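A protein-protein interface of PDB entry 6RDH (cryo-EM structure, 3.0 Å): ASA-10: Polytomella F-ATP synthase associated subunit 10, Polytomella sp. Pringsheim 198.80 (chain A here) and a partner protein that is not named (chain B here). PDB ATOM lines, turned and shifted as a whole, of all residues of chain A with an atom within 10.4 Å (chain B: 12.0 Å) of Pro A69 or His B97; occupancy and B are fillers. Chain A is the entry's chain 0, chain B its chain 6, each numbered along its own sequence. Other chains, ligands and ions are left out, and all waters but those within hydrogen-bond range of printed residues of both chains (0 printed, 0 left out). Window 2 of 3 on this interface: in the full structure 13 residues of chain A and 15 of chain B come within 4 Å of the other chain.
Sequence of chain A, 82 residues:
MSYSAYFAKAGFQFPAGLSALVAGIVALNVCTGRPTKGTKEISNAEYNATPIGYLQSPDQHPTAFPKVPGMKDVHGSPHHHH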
ATOM      1  N   ASP A  59      19.220 -19.662 -20.457  1.00  0.00           N
ATOM      2  CA  ASP A  59      19.522 -18.410 -19.774  1.00  0.00           C
ATOM      3  C   ASP A  59      19.227 -18.499 -18.286  1.00  0.00           C
ATOM      4  O   ASP A  59      19.982 -17.963 -17.468  1.00  0.00           O
ATOM      5  CB  ASP A  59      18.716 -17.271 -20.389  1.00  0.00           C
ATOM      6  CG  ASP A  59      19.268 -16.816 -21.707  1.00  0.00           C
ATOM      7  OD1 ASP A  59      20.506 -16.747 -21.834  1.00  0.00           O
ATOM      8  OD2 ASP A  59      18.467 -16.523 -22.615  1.00  0.00           O
ATOM      9  N   HIS A  61      19.418 -20.870 -16.176  1.00  0.00           N
ATOM     10  CA  HIS A  61      20.280 -21.733 -15.371  1.00  0.00           C
ATOM     11  C   HIS A  61      21.740 -21.424 -15.663  1.00  0.00           C
ATOM     12  O   HIS A  61      22.421 -22.203 -16.335  1.00  0.00           O
ATOM     13  CB  HIS A  61      19.984 -23.205 -15.648  1.00  0.00           C
ATOM     14  CG  HIS A  61      18.569 -23.599 -15.387  1.00  0.00           C
ATOM     15  ND1 HIS A  61      18.191 -24.312 -14.273  1.00  0.00           N
ATOM     16  CD2 HIS A  61      17.440 -23.389 -16.100  1.00  0.00           C
ATOM     17  CE1 HIS A  61      16.888 -24.517 -14.306  1.00  0.00           C
ATOM     18  NE2 HIS A  61      16.407 -23.966 -15.405  1.00  0.00           N
ATOM     19  N   PRO A  62      22.263 -20.306 -15.170  1.00  0.00           N
ATOM     20  CA  PRO A  62      23.678 -20.022 -15.374  1.00  0.00           C
ATOM     21  C   PRO A  62      24.540 -20.821 -14.414  1.00  0.00           C
ATOM     22  O   PRO A  62      24.100 -21.256 -13.352  1.00  0.00           O
ATOM     23  CB  PRO A  62      23.778 -18.525 -15.096  1.00  0.00           C
ATOM     24  CG  PRO A  62      22.727 -18.272 -14.141  1.00  0.00           C
ATOM     25  CD  PRO A  62      21.613 -19.219 -14.423  1.00  0.00           C
ATOM     26  N   THR A  63      25.788 -21.013 -14.824  1.00  0.00           N
ATOM     27  CA  THR A  63      26.715 -21.859 -14.092  1.00  0.00           C
ATOM     28  C   THR A  63      27.151 -21.157 -12.816  1.00  0.00           C
ATOM     29  O   THR A  63      27.413 -19.953 -12.816  1.00  0.00           O
ATOM     30  CB  THR A  63      27.904 -22.203 -14.989  1.00  0.00           C
ATOM     31  OG1 THR A  63      27.439 -23.036 -16.054  1.00  0.00           O
ATOM     32  CG2 THR A  63      28.995 -22.949 -14.249  1.00  0.00           C
ATOM     33  N   ALA A  64      27.189 -21.923 -11.720  1.00  0.00           N
ATOM     34  CA  ALA A  64      27.355 -21.362 -10.387  1.00  0.00           C
ATOM     35  C   ALA A  64      28.708 -20.702 -10.185  1.00  0.00           C
ATOM     36  O   ALA A  64      28.827 -19.796  -9.369  1.00  0.00           O
ATOM     37  CB  ALA A  64      27.149 -22.450  -9.339  1.00  0.00           C
ATOM     38  N   PHE A  65      29.734 -21.133 -10.900  1.00  0.00           N
ATOM     39  CA  PHE A  65      31.046 -20.490 -10.835  1.00  0.00           C
ATOM     40  C   PHE A  65      31.673 -20.616 -12.204  1.00  0.00           C
ATOM     41  O   PHE A  65      32.545 -21.463 -12.429  1.00  0.00           O
ATOM     42  CB  PHE A  65      31.937 -21.140  -9.781  1.00  0.00           C
ATOM     43  CG  PHE A  65      31.763 -20.592  -8.402  1.00  0.00           C
ATOM     44  CD1 PHE A  65      32.492 -19.502  -7.986  1.00  0.00           C
ATOM     45  CD2 PHE A  65      30.906 -21.200  -7.506  1.00  0.00           C
ATOM     46  CE1 PHE A  65      32.350 -19.009  -6.718  1.00  0.00           C
ATOM     47  CE2 PHE A  65      30.753 -20.701  -6.239  1.00  0.00           C
ATOM     48  CZ  PHE A  65      31.479 -19.604  -5.843  1.00  0.00           C
ATOM     49  N   PRO A  66      31.251 -19.785 -13.156  1.00  0.00           N
ATOM     50  CA  PRO A  66      31.531 -20.071 -14.566  1.00  0.00           C
ATOM     51  C   PRO A  66      32.990 -19.840 -14.909  1.00  0.00           C
ATOM     52  O   PRO A  66      33.571 -18.813 -14.558  1.00  0.00           O
ATOM     53  CB  PRO A  66      30.616 -19.098 -15.311  1.00  0.00           C
ATOM     54  CG  PRO A  66      30.397 -17.996 -14.376  1.00  0.00           C
ATOM     55  CD  PRO A  66      30.439 -18.572 -12.994  1.00  0.00           C
ATOM     56  N   LYS A  67      33.591 -20.828 -15.570  1.00  0.00           N
ATOM     57  CA  LYS A  67      34.950 -20.653 -16.056  1.00  0.00           C
ATOM     58  C   LYS A  67      34.981 -19.727 -17.257  1.00  0.00           C
ATOM     59  O   LYS A  67      35.972 -19.032 -17.479  1.00  0.00           O
ATOM     60  CB  LYS A  67      35.560 -22.004 -16.401  1.00  0.00           C
ATOM     61  CG  LYS A  67      35.592 -22.981 -15.247  1.00  0.00           C
ATOM     62  CD  LYS A  67      36.481 -22.493 -14.129  1.00  0.00           C
ATOM     63  CE  LYS A  67      36.777 -23.602 -13.158  1.00  0.00           C
ATOM     64  NZ  LYS A  67      37.781 -23.194 -12.161  1.00  0.00           N
ATOM     65  N   VAL A  68      33.906 -19.697 -18.034  1.00  0.00           N
ATOM     66  CA  VAL A  68      33.751 -18.774 -19.148  1.00  0.00           C
ATOM     67  C   VAL A  68      32.473 -17.985 -18.908  1.00  0.00           C
ATOM     68  O   VAL A  68      31.428 -18.587 -18.659  1.00  0.00           O
ATOM     69  CB  VAL A  68      33.691 -19.498 -20.503  1.00  0.00           C
ATOM     70  CG1 VAL A  68      33.344 -18.529 -21.598  1.00  0.00           C
ATOM     71  CG2 VAL A  68      35.017 -20.146 -20.785  1.00  0.00           C
ATOM     72  N   PRO A  69      32.516 -16.651 -18.934  1.00  0.00           N
ATOM     73  CA  PRO A  69      31.313 -15.854 -18.679  1.00  0.00           C
ATOM     74  C   PRO A  69      30.230 -16.057 -19.721  1.00  0.00           C
ATOM     75  O   PRO A  69      30.379 -15.664 -20.880  1.00  0.00           O
ATOM     76  CB  PRO A  69      31.843 -14.419 -18.700  1.00  0.00           C
ATOM     77  CG  PRO A  69      33.278 -14.551 -18.371  1.00  0.00           C
ATOM     78  CD  PRO A  69      33.720 -15.813 -18.996  1.00  0.00           C
ATOM     79  N   GLY A  70      29.134 -16.674 -19.301  1.00  0.00           N
ATOM     80  CA  GLY A  70      28.088 -17.121 -20.196  1.00  0.00           C
ATOM     81  C   GLY A  70      27.831 -18.607 -20.138  1.00  0.00           C
ATOM     82  O   GLY A  70      26.929 -19.084 -20.837  1.00  0.00           O
ATOM     83  N   MET A  71      28.591 -19.360 -19.344  1.00  0.00           N
ATOM     84  CA  MET A  71      28.384 -20.795 -19.208  1.00  0.00           C
ATOM     85  C   MET A  71      27.066 -21.072 -18.510  1.00  0.00           C
ATOM     86  O   MET A  71      26.732 -20.425 -17.517  1.00  0.00           O
ATOM     87  CB  MET A  71      29.524 -21.423 -18.413  1.00  0.00           C
ATOM     88  CG  MET A  71      30.735 -21.790 -19.226  1.00  0.00           C
ATOM     89  SD  MET A  71      32.177 -22.106 -18.199  1.00  0.00           S
ATOM     90  CE  MET A  71      31.531 -23.323 -17.068  1.00  0.00           C
ATOM     91  N   LYS A  72      26.305 -22.021 -19.039  1.00  0.00           N
ATOM     92  CA  LYS A  72      25.004 -22.374 -18.499  1.00  0.00           C
ATOM     93  C   LYS A  72      24.984 -23.852 -18.143  1.00  0.00           C
ATOM     94  O   LYS A  72      25.782 -24.643 -18.645  1.00  0.00           O
ATOM     95  CB  LYS A  72      23.888 -22.063 -19.495  1.00  0.00           C
ATOM     96  CG  LYS A  72      23.999 -20.698 -20.149  1.00  0.00           C
ATOM     97  CD  LYS A  72      23.917 -19.598 -19.113  1.00  0.00           C
ATOM     98  CE  LYS A  72      23.932 -18.225 -19.739  1.00  0.00           C
ATOM     99  NZ  LYS A  72      23.931 -17.172 -18.700  1.00  0.00           N
ATOM    100  N   ARG B  89      22.141 -15.225  -1.131  1.00  0.00           N
ATOM    101  CA  ARG B  89      22.756 -14.101  -1.821  1.00  0.00           C
ATOM    102  C   ARG B  89      24.115 -14.465  -2.394  1.00  0.00           C
ATOM    103  O   ARG B  89      24.511 -13.908  -3.415  1.00  0.00           O
ATOM    104  CB  ARG B  89      22.891 -12.918  -0.875  1.00  0.00           C
ATOM    105  CG  ARG B  89      21.591 -12.269  -0.509  1.00  0.00           C
ATOM    106  CD  ARG B  89      21.045 -11.462  -1.631  1.00  0.00           C
ATOM    107  NE  ARG B  89      22.041 -10.539  -2.139  1.00  0.00           N
ATOM    108  CZ  ARG B  89      21.751  -9.508  -2.911  1.00  0.00           C
ATOM    109  NH1 ARG B  89      20.494  -9.273  -3.242  1.00  0.00           N
ATOM    110  NH2 ARG B  89      22.712  -8.717  -3.346  1.00  0.00           N
ATOM    111  N   ALA B  90      24.838 -15.398  -1.776  1.00  0.00           N
ATOM    112  CA  ALA B  90      26.111 -15.817  -2.342  1.00  0.00           C
ATOM    113  C   ALA B  90      25.932 -16.797  -3.490  1.00  0.00           C
ATOM    114  O   ALA B  90      26.798 -16.878  -4.362  1.00  0.00           O
ATOM    115  CB  ALA B  90      26.993 -16.433  -1.266  1.00  0.00           C
ATOM    116  N   ASP B  91      24.843 -17.563  -3.497  1.00  0.00           N
ATOM    117  CA  ASP B  91      24.509 -18.343  -4.682  1.00  0.00           C
ATOM    118  C   ASP B  91      24.136 -17.429  -5.835  1.00  0.00           C
ATOM    119  O   ASP B  91      24.522 -17.673  -6.979  1.00  0.00           O
ATOM    120  CB  ASP B  91      23.366 -19.319  -4.396  1.00  0.00           C
ATOM    121  CG  ASP B  91      23.719 -20.356  -3.343  1.00  0.00           C
ATOM    122  OD1 ASP B  91      22.801 -21.064  -2.873  1.00  0.00           O
ATOM    123  OD2 ASP B  91      24.908 -20.467  -2.978  1.00  0.00           O
ATOM    124  N   GLY B  92      23.386 -16.366  -5.554  1.00  0.00           N
ATOM    125  CA  GLY B  92      23.011 -15.444  -6.611  1.00  0.00           C
ATOM    126  C   GLY B  92      24.124 -14.526  -7.077  1.00  0.00           C
ATOM    127  O   GLY B  92      24.090 -14.072  -8.220  1.00  0.00           O
ATOM    128  N   GLN B  93      25.097 -14.229  -6.217  1.00  0.00           N
ATOM    129  CA  GLN B  93      26.217 -13.395  -6.637  1.00  0.00           C
ATOM    130  C   GLN B  93      27.173 -14.159  -7.520  1.00  0.00           C
ATOM    131  O   GLN B  93      27.811 -13.577  -8.401  1.00  0.00           O
ATOM    132  CB  GLN B  93      26.986 -12.852  -5.440  1.00  0.00           C
ATOM    133  CG  GLN B  93      26.384 -11.660  -4.776  1.00  0.00           C
ATOM    134  CD  GLN B  93      27.246 -11.169  -3.658  1.00  0.00           C
ATOM    135  OE1 GLN B  93      28.218 -11.810  -3.287  1.00  0.00           O
ATOM    136  NE2 GLN B  93      26.923  -9.997  -3.137  1.00  0.00           N
ATOM    137  N   SER B  94      27.307 -15.454  -7.293  1.00  0.00           N
ATOM    138  CA  SER B  94      28.333 -16.209  -7.985  1.00  0.00           C
ATOM    139  C   SER B  94      27.929 -16.609  -9.392  1.00  0.00           C
ATOM    140  O   SER B  94      28.777 -17.093 -10.137  1.00  0.00           O
ATOM    141  CB  SER B  94      28.695 -17.443  -7.176  1.00  0.00           C
ATOM    142  OG  SER B  94      27.609 -18.343  -7.152  1.00  0.00           O
ATOM    143  N   LYS B  95      26.687 -16.391  -9.795  1.00  0.00           N
ATOM    144  CA  LYS B  95      26.260 -16.683 -11.154  1.00  0.00           C
ATOM    145  C   LYS B  95      25.709 -15.437 -11.839  1.00  0.00           C
ATOM    146  O   LYS B  95      24.706 -15.491 -12.548  1.00  0.00           O
ATOM    147  CB  LYS B  95      25.240 -17.815 -11.166  1.00  0.00           C
ATOM    148  CG  LYS B  95      24.075 -17.632 -10.229  1.00  0.00           C
ATOM    149  CD  LYS B  95      23.169 -18.849 -10.195  1.00  0.00           C
ATOM    150  CE  LYS B  95      23.776 -19.957  -9.375  1.00  0.00           C
ATOM    151  NZ  LYS B  95      22.775 -20.993  -9.042  1.00  0.00           N
ATOM    152  N   ALA B  96      26.381 -14.299 -11.679  1.00  0.00           N
ATOM    153  CA  ALA B  96      25.790 -13.020 -12.052  1.00  0.00           C
ATOM    154  C   ALA B  96      26.476 -12.328 -13.222  1.00  0.00           C
ATOM    155  O   ALA B  96      26.245 -11.127 -13.414  1.00  0.00           O
ATOM    156  CB  ALA B  96      25.789 -12.081 -10.845  1.00  0.00           C
ATOM    157  N   HIS B  97      27.361 -13.028 -13.948  1.00  0.00           N
ATOM    158  CA  HIS B  97      28.126 -12.607 -15.133  1.00  0.00           C
ATOM    159  C   HIS B  97      29.240 -11.619 -14.784  1.00  0.00           C
ATOM    160  O   HIS B  97      30.190 -11.453 -15.548  1.00  0.00           O
ATOM    161  CB  HIS B  97      27.184 -12.049 -16.229  1.00  0.00           C
ATOM    162  CG  HIS B  97      27.878 -11.351 -17.361  1.00  0.00           C
ATOM    163  ND1 HIS B  97      29.052 -11.812 -17.914  1.00  0.00           N
ATOM    164  CD2 HIS B  97      27.589 -10.198 -18.005  1.00  0.00           C
ATOM    165  CE1 HIS B  97      29.443 -10.984 -18.863  1.00  0.00           C
ATOM    166  NE2 HIS B  97      28.571  -9.997 -18.942  1.00  0.00           N
ATOM    167  N   GLU B  98      29.226 -11.072 -13.584  1.00  0.00           N
ATOM    168  CA  GLU B  98      30.292 -10.232 -13.072  1.00  0.00           C
ATOM    169  C   GLU B  98      30.663 -10.760 -11.701  1.00  0.00           C
ATOM    170  O   GLU B  98      30.805 -10.034 -10.718  1.00  0.00           O
ATOM    171  CB  GLU B  98      29.827  -8.778 -13.058  1.00  0.00           C
ATOM    172  CG  GLU B  98      30.911  -7.715 -12.955  1.00  0.00           C
ATOM    173  CD  GLU B  98      31.715  -7.550 -14.235  1.00  0.00           C
ATOM    174  OE1 GLU B  98      31.178  -7.843 -15.325  1.00  0.00           O
ATOM    175  OE2 GLU B  98      32.882  -7.112 -14.151  1.00  0.00           O
ATOM    176  N   TRP B  99      30.791 -12.085 -11.644  1.00  0.00           N
ATOM    177  CA  TRP B  99      30.618 -12.828 -10.403  1.00  0.00           C
ATOM    178  C   TRP B  99      31.811 -12.683  -9.476  1.00  0.00           C
ATOM    179  O   TRP B  99      31.638 -12.544  -8.260  1.00  0.00           O
ATOM    180  CB  TRP B  99      30.364 -14.296 -10.728  1.00  0.00           C
ATOM    181  CG  TRP B  99      31.422 -14.911 -11.584  1.00  0.00           C
ATOM    182  CD1 TRP B  99      31.524 -14.848 -12.939  1.00  0.00           C
ATOM    183  CD2 TRP B  99      32.537 -15.680 -11.136  1.00  0.00           C
ATOM    184  NE1 TRP B  99      32.634 -15.523 -13.362  1.00  0.00           N
ATOM    185  CE2 TRP B  99      33.272 -16.043 -12.269  1.00  0.00           C
ATOM    186  CE3 TRP B  99      32.985 -16.092  -9.885  1.00  0.00           C
ATOM    187  CZ2 TRP B  99      34.424 -16.799 -12.187  1.00  0.00           C
ATOM    188  CZ3 TRP B  99      34.125 -16.837  -9.809  1.00  0.00           C
ATOM    189  CH2 TRP B  99      34.832 -17.185 -10.948  1.00  0.00           C
ATOM    190  N   ILE B 100      33.027 -12.708 -10.023  1.00  0.00           N
ATOM    191  CA  ILE B 100      34.207 -12.581  -9.182  1.00  0.00           C
ATOM    192  C   ILE B 100      34.309 -11.161  -8.654  1.00  0.00           C
ATOM    193  O   ILE B 100      34.786 -10.933  -7.539  1.00  0.00           O
ATOM    194  CB  ILE B 100      35.456 -13.031  -9.964  1.00  0.00           C
ATOM    195  CG1 ILE B 100      36.702 -13.028  -9.084  1.00  0.00           C
ATOM    196  CG2 ILE B 100      35.663 -12.202 -11.195  1.00  0.00           C
ATOM    197  CD1 ILE B 100      36.632 -13.986  -7.946  1.00  0.00           C
ATOM    198  N   VAL B 101      33.755 -10.203  -9.389  1.00  0.00           N
ATOM    199  CA  VAL B 101      33.702  -8.826  -8.927  1.00  0.00           C
ATOM    200  C   VAL B 101      32.761  -8.698  -7.733  1.00  0.00           C
ATOM    201  O   VAL B 101      33.069  -8.002  -6.763  1.00  0.00           O
ATOM    202  CB  VAL B 101      33.306  -7.931 -10.112  1.00  0.00           C
ATOM    203  CG1 VAL B 101      32.859  -6.586  -9.670  1.00  0.00           C
ATOM    204  CG2 VAL B 101      34.455  -7.821 -11.085  1.00  0.00           C
ATOM    205  N   ASP B 102      31.645  -9.437  -7.739  1.00  0.00           N
ATOM    206  CA  ASP B 102      30.739  -9.434  -6.590  1.00  0.00           C
ATOM    207  C   ASP B 102      31.358 -10.120  -5.381  1.00  0.00           C
ATOM    208  O   ASP B 102      31.240  -9.622  -4.249  1.00  0.00           O
ATOM    209  CB  ASP B 102      29.424 -10.119  -6.943  1.00  0.00           C
ATOM    210  CG  ASP B 102      28.671  -9.403  -8.027  1.00  0.00           C
ATOM    211  OD1 ASP B 102      29.275  -8.542  -8.687  1.00  0.00           O
ATOM    212  OD2 ASP B 102      27.472  -9.691  -8.217  1.00  0.00           O
ATOM    213  N   LEU B 103      32.017 -11.263  -5.597  1.00  0.00           N
ATOM    214  CA  LEU B 103      32.644 -11.969  -4.485  1.00  0.00           C
ATOM    215  C   LEU B 103      33.786 -11.172  -3.880  1.00  0.00           C
ATOM    216  O   LEU B 103      34.077 -11.318  -2.693  1.00  0.00           O
ATOM    217  CB  LEU B 103      33.156 -13.329  -4.932  1.00  0.00           C
ATOM    218  CG  LEU B 103      32.132 -14.297  -5.499  1.00  0.00           C
ATOM    219  CD1 LEU B 103      32.844 -15.567  -5.849  1.00  0.00           C
ATOM    220  CD2 LEU B 103      31.007 -14.553  -4.526  1.00  0.00           C
ATOM    221  N   ASN B 104      34.424 -10.313  -4.662  1.00  0.00           N
ATOM    222  CA  ASN B 104      35.438  -9.439  -4.100  1.00  0.00           C
ATOM    223  C   ASN B 104      34.868  -8.153  -3.520  1.00  0.00           C
ATOM    224  O   ASN B 104      35.506  -7.538  -2.661  1.00  0.00           O
ATOM    225  CB  ASN B 104      36.472  -9.160  -5.172  1.00  0.00           C
ATOM    226  CG  ASN B 104      37.328 -10.362  -5.441  1.00  0.00           C
ATOM    227  OD1 ASN B 104      36.841 -11.442  -5.738  1.00  0.00           O
ATOM    228  ND2 ASN B 104      38.608 -10.183  -5.349  1.00  0.00           N
ATOM    229  N   LEU B 105      33.673  -7.747  -3.940  1.00  0.00           N
ATOM    230  CA  LEU B 105      33.019  -6.629  -3.272  1.00  0.00           C
ATOM    231  C   LEU B 105      32.553  -7.007  -1.880  1.00  0.00           C
ATOM    232  O   LEU B 105      32.523  -6.151  -0.989  1.00  0.00           O
ATOM    233  CB  LEU B 105      31.850  -6.132  -4.105  1.00  0.00           C
ATOM    234  CG  LEU B 105      32.275  -5.182  -5.214  1.00  0.00           C
ATOM    235  CD1 LEU B 105      31.069  -4.667  -5.937  1.00  0.00           C
ATOM    236  CD2 LEU B 105      33.055  -4.045  -4.638  1.00  0.00           C
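The side-chain hydroxyl of Ser B94 is in hydrogen-bond range of the backbone carbonyl oxygen of Ala A64, at 2.9 Å.
The backbone NH (N) of Thr A63 is in hydrogen-bond range of the backbone carbonyl oxygen (O) of Met A71.
The side-chain hydroxyl of Thr A63 lies close to the backbone NH of Lys A72 (3.4 Å).
The backbone carbonyl oxygen (O) of Ala B90 is in hydrogen-bond range of the side-chain hydroxyl (OG) of Ser B94 (3.3 Å).
The backbone carbonyl oxygen of Asp B91 is in hydrogen-bond range of the side-chain hydroxyl of Ser B94 (3.2 Å).
Among the printed residues, pairs that only touch across the chains: Pro A62 with Lys B95 (3.8 Å), Thr A63 with Lys B95 (3.5 Å), Ala A64 with Lys B95 (3.98 Å), Phe A65 with Ser B94 (3.8 Å), Phe A65 with Trp B99 (3.6 Å), Phe A65 with Leu B103 (3.6 Å), Pro A66 with Ser B94 (3.6 Å), Pro A66 with Trp B99 (3.2 Å) and Pro A69 with His B97 (3.9 Å).
Pro A69 touches one residue of chain B.
Of chain A, only Pro A69 comes within 4 Å of His B97.
Of the printed residues of chain B, Pro A66 touches Ser B94 and Trp B99.
No residue of chain B comes within 4 Å of Gly A70.
No residue of chain B comes within 4 Å of Met A71.
No residue of chain A comes within 4 Å of Ala B96.
Of the printed residues of chain B, Pro A62 touches Lys B95.
Of the printed residues of chain A, Trp B99 touches Phe A65 and Pro A66.
His A61 touches none of the printed residues of chain B.
The nearest residue of chain A that does not touch His B97 is Gly A70 (5.1 Å).
Hydrophobic or aromatic side chains of chain B that line the printed part of chain A: His B97, Trp B99 and Leu B103.
Of the 13 printed residues of chain A, 6 touch a printed residue of chain B.
Hydrophobic or aromatic side chains of chain A that line the printed part of chain B: Pro A62, Phe A65, Pro A66 and Pro A69.
Among the printed residues, 10 pairs touch across the chains.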
